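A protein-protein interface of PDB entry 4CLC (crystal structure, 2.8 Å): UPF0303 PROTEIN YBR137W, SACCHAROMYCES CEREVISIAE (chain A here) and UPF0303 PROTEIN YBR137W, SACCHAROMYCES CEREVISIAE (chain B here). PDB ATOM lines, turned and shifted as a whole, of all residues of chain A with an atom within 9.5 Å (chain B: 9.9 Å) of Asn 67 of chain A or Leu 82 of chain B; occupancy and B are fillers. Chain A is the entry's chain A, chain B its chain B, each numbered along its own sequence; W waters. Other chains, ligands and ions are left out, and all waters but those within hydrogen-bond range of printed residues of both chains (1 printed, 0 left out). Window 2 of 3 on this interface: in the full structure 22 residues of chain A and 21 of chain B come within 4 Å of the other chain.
NH1 of Arg 73 of chain B is in salt-bridge range of OD2 of Asp 85 of chain B, 3.2 Å away. The backbone carbonyl oxygen of Ile 63 of chain A lies within hydrogen-bond range of the backbone NH of Leu 71 of chain A (2.9 Å). The backbone NH of Ala 81 of chain B sits close to the side-chain amide nitrogen of Asn 84 of chain B, 3.4 Å away. N of His 69 of chain A sits at hydrogen-bond distance from OD1 of Asn 67 of chain A, 3.3 Å away.
No residue of chain B comes within 4 Å of Leu 65 of chain A. No residue of chain B comes within 4 Å of Pro 66 of chain A. Of chain B, only Leu 82 (3.5 Å) comes within 4 Å of Asn 67 of chain A. Gly 68 of chain A touches just one residue of chain B: Leu 82. Of chain B, only Ser 80 (2.8 Å), Ala 81 (3.1 Å), Leu 82 (3.5 Å) and Asp 85 (2.7 Å) come within 4 Å of His 69 of chain A. Of the printed residues of chain B, Cys 70 of chain A touches Arg 73 (3.8 Å) and Asp 85 (3.4 Å). Printed residues of chain B within 4 Å of Leu 71 of chain A: Arg 73 (3.7 Å) and Val 75 (3.7 Å). Ala 144 of chain A touches none of the printed residues of chain B. Of the printed residues of chain A, Arg 73 of chain B touches Cys 70 (3.8 Å) and Leu 71 (3.7 Å). Of the printed residues of chain A, Val 75 of chain B touches Leu 71 (3.7 Å). Of the printed residues of chain A, Ser 80 of chain B touches His 69 (2.8 Å). Of the printed residues of chain A, Ala 81 of chain B touches His 69. Gln 89 of chain B touches none of the printed residues of chain A. The nearest residue of chain B that does not touch Asn 67 of chain A is Ala 81 of chain B (5.6 Å).
Water W1 lies within hydrogen-bond range of NH1 of Arg 73 of chain B (2.6 Å), OD1 of Asp 85 of chain B (2.9 Å) and O of Cys 70 of chain A (3.1 Å).
CD2 of Leu 82 of chain B touches O of Asn 67 of chain A, at 3.5 Å. C of Gly 68 of chain A touches CD1 of Leu 82 of chain B, at 3.7 Å. Leu 82 of chain B touches His 69 of chain A (CD1 to N, 3.5 Å). O of Cys 70 of chain A touches CG of Arg 73 of chain B, at 3.8 Å. O of Leu 71 of chain A touches O of Arg 73 of chain B, 3.7 Å away. O of Leu 71 of chain A touches CG1 of Val 75 of chain B, at 3.7 Å.
Of the 17 printed residues of chain A, 5 touch a printed residue of chain B. Printed residues of chain A that touch a printed residue of chain B: Asn 67, Gly 68, His 69, Cys 70 and Leu 71. Hydrophobic or aromatic side chains of chain A within 4 Å of the printed part of chain B: His 69 and Leu 71. Printed residues of chain B that touch a printed residue of chain A: Arg 73, Val 75, Ser 80, Ala 81, Leu 82 and Asp 85. Hydrophobic or aromatic side chains of chain B that line the printed part of chain A: Val 75 and Leu 82. Among the printed residues, no Asp or Glu carboxylate lies within 4 Å of a Lys or Arg side-chain nitrogen of the other chain.
The side-chain hydroxyl (OG) of Ser 80 of chain B is in hydrogen-bond range of a ring nitrogen (NE2) of His 69 of chain A, 2.8 Å away. OD1 of Asp 85 of chain B is in hydrogen-bond range of N of Cys 70 of chain A, at 3.4 Å. OD1 of Asp 85 of chain B is in hydrogen-bond range of ND1 of His 69 of chain A (2.7 Å). A ring nitrogen (ND1) of His 69 of chain A lies close to the backbone carbonyl oxygen (O) of Ala 81 of chain B, at 3.2 Å.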
ATOM      1  N   PHE A  34     -30.607   8.430   6.897  1.00  0.00           N
ATOM      2  CA  PHE A  34     -29.443   7.870   7.564  1.00  0.00           C
ATOM      3  C   PHE A  34     -29.940   6.960   8.672  1.00  0.00           C
ATOM      4  O   PHE A  34     -30.463   7.434   9.677  1.00  0.00           O
ATOM      5  CB  PHE A  34     -28.558   8.984   8.120  1.00  0.00           C
ATOM      6  CG  PHE A  34     -27.268   8.505   8.715  1.00  0.00           C
ATOM      7  CD1 PHE A  34     -26.144   8.321   7.917  1.00  0.00           C
ATOM      8  CD2 PHE A  34     -27.171   8.258  10.072  1.00  0.00           C
ATOM      9  CE1 PHE A  34     -24.944   7.889   8.458  1.00  0.00           C
ATOM     10  CE2 PHE A  34     -25.979   7.833  10.625  1.00  0.00           C
ATOM     11  CZ  PHE A  34     -24.861   7.647   9.817  1.00  0.00           C
ATOM     12  N   ILE A  63     -17.535   4.832  10.539  1.00  0.00           N
ATOM     13  CA  ILE A  63     -18.657   5.750  10.600  1.00  0.00           C
ATOM     14  C   ILE A  63     -19.126   5.878  12.042  1.00  0.00           C
ATOM     15  O   ILE A  63     -19.529   4.891  12.665  1.00  0.00           O
ATOM     16  CB  ILE A  63     -19.832   5.312   9.725  1.00  0.00           C
ATOM     17  CG1 ILE A  63     -19.381   5.051   8.286  1.00  0.00           C
ATOM     18  CG2 ILE A  63     -20.906   6.391   9.740  1.00  0.00           C
ATOM     19  CD1 ILE A  63     -20.495   4.506   7.378  1.00  0.00           C
ATOM     20  N   SER A  64     -19.072   7.103  12.561  1.00  0.00           N
ATOM     21  CA  SER A  64     -19.433   7.395  13.946  1.00  0.00           C
ATOM     22  C   SER A  64     -20.407   8.562  14.012  1.00  0.00           C
ATOM     23  O   SER A  64     -20.377   9.430  13.140  1.00  0.00           O
ATOM     24  CB  SER A  64     -18.185   7.730  14.774  1.00  0.00           C
ATOM     25  OG  SER A  64     -17.466   6.574  15.165  1.00  0.00           O
ATOM     26  N   LEU A  65     -21.252   8.586  15.045  1.00  0.00           N
ATOM     27  CA  LEU A  65     -22.130   9.730  15.315  1.00  0.00           C
ATOM     28  C   LEU A  65     -21.346  10.825  16.030  1.00  0.00           C
ATOM     29  O   LEU A  65     -20.296  10.545  16.612  1.00  0.00           O
ATOM     30  CB  LEU A  65     -23.332   9.315  16.161  1.00  0.00           C
ATOM     31  CG  LEU A  65     -24.241   8.200  15.645  1.00  0.00           C
ATOM     32  CD1 LEU A  65     -25.370   7.970  16.639  1.00  0.00           C
ATOM     33  CD2 LEU A  65     -24.779   8.504  14.250  1.00  0.00           C
ATOM     34  N   PRO A  66     -21.841  12.078  15.994  1.00  0.00           N
ATOM     35  CA  PRO A  66     -21.113  13.179  16.648  1.00  0.00           C
ATOM     36  C   PRO A  66     -20.907  13.011  18.159  1.00  0.00           C
ATOM     37  O   PRO A  66     -20.074  13.724  18.713  1.00  0.00           O
ATOM     38  CB  PRO A  66     -21.996  14.413  16.366  1.00  0.00           C
ATOM     39  CG  PRO A  66     -23.292  13.882  15.825  1.00  0.00           C
ATOM     40  CD  PRO A  66     -22.964  12.577  15.181  1.00  0.00           C
ATOM     41  N   ASN A  67     -21.645  12.114  18.812  1.00  0.00           N
ATOM     42  CA  ASN A  67     -21.435  11.850  20.234  1.00  0.00           C
ATOM     43  C   ASN A  67     -20.414  10.730  20.466  1.00  0.00           C
ATOM     44  O   ASN A  67     -20.189  10.298  21.602  1.00  0.00           O
ATOM     45  CB  ASN A  67     -22.752  11.488  20.912  1.00  0.00           C
ATOM     46  CG  ASN A  67     -23.292  10.155  20.441  1.00  0.00           C
ATOM     47  OD1 ASN A  67     -23.062   9.749  19.299  1.00  0.00           O
ATOM     48  ND2 ASN A  67     -24.003   9.456  21.322  1.00  0.00           N
ATOM     49  N   GLY A  68     -19.820  10.239  19.383  1.00  0.00           N
ATOM     50  CA  GLY A  68     -18.821   9.192  19.482  1.00  0.00           C
ATOM     51  C   GLY A  68     -19.304   7.766  19.251  1.00  0.00           C
ATOM     52  O   GLY A  68     -18.499   6.872  18.969  1.00  0.00           O
ATOM     53  N   HIS A  69     -20.610   7.544  19.365  1.00  0.00           N
ATOM     54  CA  HIS A  69     -21.166   6.215  19.150  1.00  0.00           C
ATOM     55  C   HIS A  69     -20.823   5.666  17.756  1.00  0.00           C
ATOM     56  O   HIS A  69     -21.191   6.236  16.721  1.00  0.00           O
ATOM     57  CB  HIS A  69     -22.678   6.239  19.344  1.00  0.00           C
ATOM     58  CG  HIS A  69     -23.329   4.911  19.130  1.00  0.00           C
ATOM     59  ND1 HIS A  69     -22.777   3.729  19.581  1.00  0.00           N
ATOM     60  CD2 HIS A  69     -24.487   4.571  18.516  1.00  0.00           C
ATOM     61  CE1 HIS A  69     -23.569   2.725  19.253  1.00  0.00           C
ATOM     62  NE2 HIS A  69     -24.613   3.207  18.610  1.00  0.00           N
ATOM     63  N   CYS A  70     -20.159   4.518  17.752  1.00  0.00           N
ATOM     64  CA  CYS A  70     -19.594   3.965  16.531  1.00  0.00           C
ATOM     65  C   CYS A  70     -20.526   2.962  15.846  1.00  0.00           C
ATOM     66  O   CYS A  70     -20.779   1.879  16.374  1.00  0.00           O
ATOM     67  CB  CYS A  70     -18.260   3.297  16.850  1.00  0.00           C
ATOM     68  SG  CYS A  70     -17.323   2.761  15.422  1.00  0.00           S
ATOM     69  N   LEU A  71     -21.032   3.343  14.673  1.00  0.00           N
ATOM     70  CA  LEU A  71     -21.896   2.494  13.848  1.00  0.00           C
ATOM     71  C   LEU A  71     -21.167   1.478  12.953  1.00  0.00           C
ATOM     72  O   LEU A  71     -21.602   0.326  12.817  1.00  0.00           O
ATOM     73  CB  LEU A  71     -22.770   3.374  12.973  1.00  0.00           C
ATOM     74  CG  LEU A  71     -23.571   4.415  13.745  1.00  0.00           C
ATOM     75  CD1 LEU A  71     -24.203   5.359  12.748  1.00  0.00           C
ATOM     76  CD2 LEU A  71     -24.625   3.755  14.621  1.00  0.00           C
ATOM     77  N   GLN A  89      -9.532   8.542  15.445  1.00  0.00           N
ATOM     78  CA  GLN A  89     -10.001   9.352  16.560  1.00  0.00           C
ATOM     79  C   GLN A  89      -9.629  10.804  16.362  1.00  0.00           C
ATOM     80  O   GLN A  89     -10.468  11.694  16.494  1.00  0.00           O
ATOM     81  CB  GLN A  89      -9.427   8.846  17.889  1.00  0.00           C
ATOM     82  CG  GLN A  89     -10.022   7.537  18.336  1.00  0.00           C
ATOM     83  CD  GLN A  89     -11.517   7.637  18.615  1.00  0.00           C
ATOM     84  OE1 GLN A  89     -11.941   8.293  19.575  1.00  0.00           O
ATOM     85  NE2 GLN A  89     -12.324   6.990  17.776  1.00  0.00           N
ATOM     86  N   LYS A  92     -11.314  12.426  13.073  1.00  0.00           N
ATOM     87  CA  LYS A  92     -12.744  12.575  13.342  1.00  0.00           C
ATOM     88  C   LYS A  92     -13.022  13.666  14.370  1.00  0.00           C
ATOM     89  O   LYS A  92     -14.014  14.381  14.259  1.00  0.00           O
ATOM     90  CB  LYS A  92     -13.324  11.241  13.819  1.00  0.00           C
ATOM     91  CG  LYS A  92     -14.789  11.246  14.153  1.00  0.00           C
ATOM     92  CD  LYS A  92     -15.248   9.863  14.643  1.00  0.00           C
ATOM     93  CE  LYS A  92     -14.566   9.457  15.951  1.00  0.00           C
ATOM     94  NZ  LYS A  92     -15.187   8.252  16.572  1.00  0.00           N
ATOM     95  N   LEU A  96     -15.661  16.914  13.658  1.00  0.00           N
ATOM     96  CA  LEU A  96     -16.829  17.133  14.495  1.00  0.00           C
ATOM     97  C   LEU A  96     -16.717  18.452  15.274  1.00  0.00           C
ATOM     98  O   LEU A  96     -17.714  19.140  15.501  1.00  0.00           O
ATOM     99  CB  LEU A  96     -17.021  15.957  15.441  1.00  0.00           C
ATOM    100  CG  LEU A  96     -17.381  14.622  14.776  1.00  0.00           C
ATOM    101  CD1 LEU A  96     -17.299  13.451  15.787  1.00  0.00           C
ATOM    102  CD2 LEU A  96     -18.759  14.671  14.089  1.00  0.00           C
ATOM    103  N   PRO A 142     -24.487  18.110  10.881  1.00  0.00           N
ATOM    104  CA  PRO A 142     -24.121  16.776  10.386  1.00  0.00           C
ATOM    105  C   PRO A 142     -24.828  15.624  11.069  1.00  0.00           C
ATOM    106  O   PRO A 142     -25.041  15.651  12.288  1.00  0.00           O
ATOM    107  CB  PRO A 142     -22.616  16.695  10.666  1.00  0.00           C
ATOM    108  CG  PRO A 142     -22.293  17.869  11.552  1.00  0.00           C
ATOM    109  CD  PRO A 142     -23.296  18.910  11.209  1.00  0.00           C
ATOM    110  N   TYR A 143     -25.191  14.636  10.256  1.00  0.00           N
ATOM    111  CA  TYR A 143     -25.667  13.325  10.693  1.00  0.00           C
ATOM    112  C   TYR A 143     -24.641  12.608  11.565  1.00  0.00           C
ATOM    113  O   TYR A 143     -24.930  12.142  12.671  1.00  0.00           O
ATOM    114  CB  TYR A 143     -25.955  12.430   9.477  1.00  0.00           C
ATOM    115  CG  TYR A 143     -27.355  12.462   8.886  1.00  0.00           C
ATOM    116  CD1 TYR A 143     -28.480  12.270   9.685  1.00  0.00           C
ATOM    117  CD2 TYR A 143     -27.543  12.644   7.515  1.00  0.00           C
ATOM    118  CE1 TYR A 143     -29.748  12.282   9.139  1.00  0.00           C
ATOM    119  CE2 TYR A 143     -28.800  12.653   6.963  1.00  0.00           C
ATOM    120  CZ  TYR A 143     -29.902  12.474   7.780  1.00  0.00           C
ATOM    121  OH  TYR A 143     -31.164  12.481   7.232  1.00  0.00           O
ATOM    122  N   ALA A 144     -23.438  12.498  11.013  1.00  0.00           N
ATOM    123  CA  ALA A 144     -22.388  11.662  11.554  1.00  0.00           C
ATOM    124  C   ALA A 144     -21.092  11.980  10.840  1.00  0.00           C
ATOM    125  O   ALA A 144     -21.071  12.772   9.903  1.00  0.00           O
ATOM    126  CB  ALA A 144     -22.737  10.201  11.385  1.00  0.00           C
ATOM    127  N   CYS A 145     -20.014  11.337  11.260  1.00  0.00           N
ATOM    128  CA  CYS A 145     -18.730  11.548  10.610  1.00  0.00           C
ATOM    129  C   CYS A 145     -18.262  10.265   9.946  1.00  0.00           C
ATOM    130  O   CYS A 145     -18.519   9.168  10.455  1.00  0.00           O
ATOM    131  CB  CYS A 145     -17.687  12.037  11.614  1.00  0.00           C
ATOM    132  SG  CYS A 145     -16.080  12.451  10.909  1.00  0.00           S
ATOM    133  N   ALA B  60     -24.772  -4.545  19.274  1.00  0.00           N
ATOM    134  CA  ALA B  60     -23.490  -4.118  18.736  1.00  0.00           C
ATOM    135  C   ALA B  60     -22.516  -5.286  18.713  1.00  0.00           C
ATOM    136  O   ALA B  60     -22.392  -6.009  19.708  1.00  0.00           O
ATOM    137  CB  ALA B  60     -22.930  -2.970  19.555  1.00  0.00           C
ATOM    138  N   ARG B  73     -16.556  -3.428  13.653  1.00  0.00           N
ATOM    139  CA  ARG B  73     -17.634  -3.034  14.538  1.00  0.00           C
ATOM    140  C   ARG B  73     -18.902  -2.827  13.744  1.00  0.00           C
ATOM    141  O   ARG B  73     -18.884  -2.159  12.699  1.00  0.00           O
ATOM    142  CB  ARG B  73     -17.287  -1.752  15.295  1.00  0.00           C
ATOM    143  CG  ARG B  73     -18.463  -1.100  16.027  1.00  0.00           C
ATOM    144  CD  ARG B  73     -18.752  -1.809  17.340  1.00  0.00           C
ATOM    145  NE  ARG B  73     -17.577  -1.889  18.225  1.00  0.00           N
ATOM    146  CZ  ARG B  73     -17.196  -0.943  19.091  1.00  0.00           C
ATOM    147  NH1 ARG B  73     -17.881   0.193  19.208  1.00  0.00           N
ATOM    148  NH2 ARG B  73     -16.118  -1.133  19.841  1.00  0.00           N
ATOM    149  N   VAL B  75     -23.609  -2.583  14.163  1.00  0.00           N
ATOM    150  CA  VAL B  75     -24.821  -2.569  14.962  1.00  0.00           C
ATOM    151  C   VAL B  75     -26.020  -2.973  14.076  1.00  0.00           C
ATOM    152  O   VAL B  75     -26.067  -2.628  12.888  1.00  0.00           O
ATOM    153  CB  VAL B  75     -25.025  -1.179  15.630  1.00  0.00           C
ATOM    154  CG1 VAL B  75     -24.776  -0.053  14.641  1.00  0.00           C
ATOM    155  CG2 VAL B  75     -26.402  -1.082  16.220  1.00  0.00           C
ATOM    156  N   GLY B  79     -31.661   2.584  17.599  1.00  0.00           N
ATOM    157  CA  GLY B  79     -31.829   2.527  19.037  1.00  0.00           C
ATOM    158  C   GLY B  79     -30.651   1.896  19.758  1.00  0.00           C
ATOM    159  O   GLY B  79     -30.761   1.468  20.913  1.00  0.00           O
ATOM    160  N   SER B  80     -29.518   1.818  19.075  1.00  0.00           N
ATOM    161  CA  SER B  80     -28.254   1.566  19.762  1.00  0.00           C
ATOM    162  C   SER B  80     -27.640   2.898  20.161  1.00  0.00           C
ATOM    163  O   SER B  80     -27.732   3.870  19.418  1.00  0.00           O
ATOM    164  CB  SER B  80     -27.287   0.793  18.884  1.00  0.00           C
ATOM    165  OG  SER B  80     -26.795   1.616  17.833  1.00  0.00           O
ATOM    166  N   ALA B  81     -27.017   2.953  21.329  1.00  0.00           N
ATOM    167  CA  ALA B  81     -26.466   4.213  21.812  1.00  0.00           C
ATOM    168  C   ALA B  81     -25.019   4.071  22.202  1.00  0.00           C
ATOM    169  O   ALA B  81     -24.474   2.965  22.192  1.00  0.00           O
ATOM    170  CB  ALA B  81     -27.256   4.707  22.983  1.00  0.00           C
ATOM    171  N   LEU B  82     -24.417   5.186  22.602  1.00  0.00           N
ATOM    172  CA  LEU B  82     -23.017   5.198  23.000  1.00  0.00           C
ATOM    173  C   LEU B  82     -22.762   4.202  24.117  1.00  0.00           C
ATOM    174  O   LEU B  82     -21.653   3.696  24.272  1.00  0.00           O
ATOM    175  CB  LEU B  82     -22.602   6.603  23.451  1.00  0.00           C
ATOM    176  CG  LEU B  82     -21.134   6.829  23.836  1.00  0.00           C
ATOM    177  CD1 LEU B  82     -20.197   6.561  22.652  1.00  0.00           C
ATOM    178  CD2 LEU B  82     -20.957   8.234  24.344  1.00  0.00           C
ATOM    179  N   ASP B  83     -23.797   3.920  24.900  1.00  0.00           N
ATOM    180  CA  ASP B  83     -23.645   3.073  26.074  1.00  0.00           C
ATOM    181  C   ASP B  83     -23.223   1.664  25.640  1.00  0.00           C
ATOM    182  O   ASP B  83     -22.557   0.935  26.384  1.00  0.00           O
ATOM    183  CB  ASP B  83     -24.943   3.077  26.890  1.00  0.00           C
ATOM    184  CG  ASP B  83     -24.866   2.213  28.140  1.00  0.00           C
ATOM    185  OD1 ASP B  83     -24.116   2.553  29.097  1.00  0.00           O
ATOM    186  OD2 ASP B  83     -25.594   1.199  28.174  1.00  0.00           O
ATOM    187  N   ASN B  84     -23.562   1.304  24.407  1.00  0.00           N
ATOM    188  CA  ASN B  84     -23.086   0.046  23.850  1.00  0.00           C
ATOM    189  C   ASN B  84     -21.564   0.001  23.697  1.00  0.00           C
ATOM    190  O   ASN B  84     -20.929  -0.984  24.098  1.00  0.00           O
ATOM    191  CB  ASN B  84     -23.769  -0.215  22.519  1.00  0.00           C
ATOM    192  CG  ASN B  84     -25.137  -0.845  22.695  1.00  0.00           C
ATOM    193  OD1 ASN B  84     -25.287  -1.821  23.444  1.00  0.00           O
ATOM    194  ND2 ASN B  84     -26.148  -0.283  22.023  1.00  0.00           N
ATOM    195  N   ASP B  85     -20.987   1.071  23.148  1.00  0.00           N
ATOM    196  CA  ASP B  85     -19.534   1.270  23.166  1.00  0.00           C
ATOM    197  C   ASP B  85     -18.913   1.019  24.553  1.00  0.00           C
ATOM    198  O   ASP B  85     -17.907   0.308  24.680  1.00  0.00           O
ATOM    199  CB  ASP B  85     -19.171   2.691  22.733  1.00  0.00           C
ATOM    200  CG  ASP B  85     -19.324   2.925  21.244  1.00  0.00           C
ATOM    201  OD1 ASP B  85     -20.472   2.989  20.742  1.00  0.00           O
ATOM    202  OD2 ASP B  85     -18.278   3.093  20.584  1.00  0.00           O
ATOM    203  N   PHE B  86     -19.496   1.611  25.593  1.00  0.00           N
ATOM    204  CA  PHE B  86     -18.948   1.416  26.932  1.00  0.00           C
ATOM    205  C   PHE B  86     -19.060  -0.032  27.398  1.00  0.00           C
ATOM    206  O   PHE B  86     -18.208  -0.510  28.154  1.00  0.00           O
ATOM    207  CB  PHE B  86     -19.632   2.330  27.945  1.00  0.00           C
ATOM    208  CG  PHE B  86     -19.233   3.764  27.829  1.00  0.00           C
ATOM    209  CD1 PHE B  86     -18.151   4.253  28.533  1.00  0.00           C
ATOM    210  CD2 PHE B  86     -19.946   4.631  27.023  1.00  0.00           C
ATOM    211  CE1 PHE B  86     -17.783   5.569  28.434  1.00  0.00           C
ATOM    212  CE2 PHE B  86     -19.576   5.956  26.932  1.00  0.00           C
ATOM    213  CZ  PHE B  86     -18.486   6.417  27.635  1.00  0.00           C
ATOM    214  N   TRP B  87     -20.110  -0.725  26.965  1.00  0.00           N
ATOM    215  CA  TRP B  87     -20.307  -2.103  27.392  1.00  0.00           C
ATOM    216  C   TRP B  87     -19.288  -2.981  26.707  1.00  0.00           C
ATOM    217  O   TRP B  87     -18.597  -3.788  27.357  1.00  0.00           O
ATOM    218  CB  TRP B  87     -21.732  -2.575  27.106  1.00  0.00           C
ATOM    219  CG  TRP B  87     -22.637  -2.214  28.221  1.00  0.00           C
ATOM    220  CD1 TRP B  87     -23.477  -1.148  28.281  1.00  0.00           C
ATOM    221  CD2 TRP B  87     -22.750  -2.881  29.481  1.00  0.00           C
ATOM    222  NE1 TRP B  87     -24.120  -1.116  29.492  1.00  0.00           N
ATOM    223  CE2 TRP B  87     -23.691  -2.174  30.247  1.00  0.00           C
ATOM    224  CE3 TRP B  87     -22.154  -4.014  30.030  1.00  0.00           C
ATOM    225  CZ2 TRP B  87     -24.056  -2.566  31.527  1.00  0.00           C
ATOM    226  CZ3 TRP B  87     -22.515  -4.398  31.309  1.00  0.00           C
ATOM    227  CH2 TRP B  87     -23.450  -3.678  32.042  1.00  0.00           C
ATOM    228  N   ILE B  88     -19.174  -2.789  25.395  1.00  0.00           N
ATOM    229  CA  ILE B  88     -18.195  -3.517  24.628  1.00  0.00           C
ATOM    230  C   ILE B  88     -16.816  -3.318  25.234  1.00  0.00           C
ATOM    231  O   ILE B  88     -16.131  -4.286  25.579  1.00  0.00           O
ATOM    232  CB  ILE B  88     -18.206  -3.082  23.173  1.00  0.00           C
ATOM    233  CG1 ILE B  88     -19.426  -3.690  22.474  1.00  0.00           C
ATOM    234  CG2 ILE B  88     -16.908  -3.526  22.482  1.00  0.00           C
ATOM    235  CD1 ILE B  88     -19.717  -3.101  21.123  1.00  0.00           C
ATOM    236  N   GLN B  89     -16.426  -2.059  25.393  1.00  0.00           N
ATOM    237  CA  GLN B  89     -15.129  -1.742  25.951  1.00  0.00           C
ATOM    238  C   GLN B  89     -14.954  -2.486  27.271  1.00  0.00           C
ATOM    239  O   GLN B  89     -13.989  -3.242  27.467  1.00  0.00           O
ATOM    240  CB  GLN B  89     -15.000  -0.232  26.140  1.00  0.00           C
ATOM    241  CG  GLN B  89     -13.570   0.264  26.338  1.00  0.00           C
ATOM    242  CD  GLN B  89     -12.691  -0.039  25.146  1.00  0.00           C
ATOM    243  OE1 GLN B  89     -13.182  -0.382  24.058  1.00  0.00           O
ATOM    244  NE2 GLN B  89     -11.376   0.062  25.342  1.00  0.00           N
ATOM    245  N   ARG B  90     -15.944  -2.308  28.140  1.00  0.00           N
ATOM    246  CA  ARG B  90     -15.883  -2.786  29.499  1.00  0.00           C
ATOM    247  C   ARG B  90     -15.822  -4.308  29.613  1.00  0.00           C
ATOM    248  O   ARG B  90     -15.004  -4.845  30.366  1.00  0.00           O
ATOM    249  CB  ARG B  90     -17.075  -2.239  30.260  1.00  0.00           C
ATOM    250  CG  ARG B  90     -16.742  -1.032  31.089  1.00  0.00           C
ATOM    251  CD  ARG B  90     -17.959  -0.249  31.488  1.00  0.00           C
ATOM    252  NE  ARG B  90     -19.083  -1.111  31.808  1.00  0.00           N
ATOM    253  CZ  ARG B  90     -19.228  -1.742  32.964  1.00  0.00           C
ATOM    254  NH1 ARG B  90     -18.315  -1.612  33.908  1.00  0.00           N
ATOM    255  NH2 ARG B  90     -20.284  -2.508  33.165  1.00  0.00           N
ATOM    256  N   SER B 149     -23.148  -6.796  22.380  1.00  0.00           N
ATOM    257  CA  SER B 149     -23.836  -6.042  23.424  1.00  0.00           C
ATOM    258  C   SER B 149     -25.281  -5.728  23.083  1.00  0.00           C
ATOM    259  O   SER B 149     -25.579  -5.369  21.945  1.00  0.00           O
ATOM    260  CB  SER B 149     -23.093  -4.731  23.702  1.00  0.00           C
ATOM    261  OG  SER B 149     -23.885  -3.822  24.456  1.00  0.00           O
HETATM  262  O   HOH W   1     -20.483   0.556  19.118  1.00  0.00           O
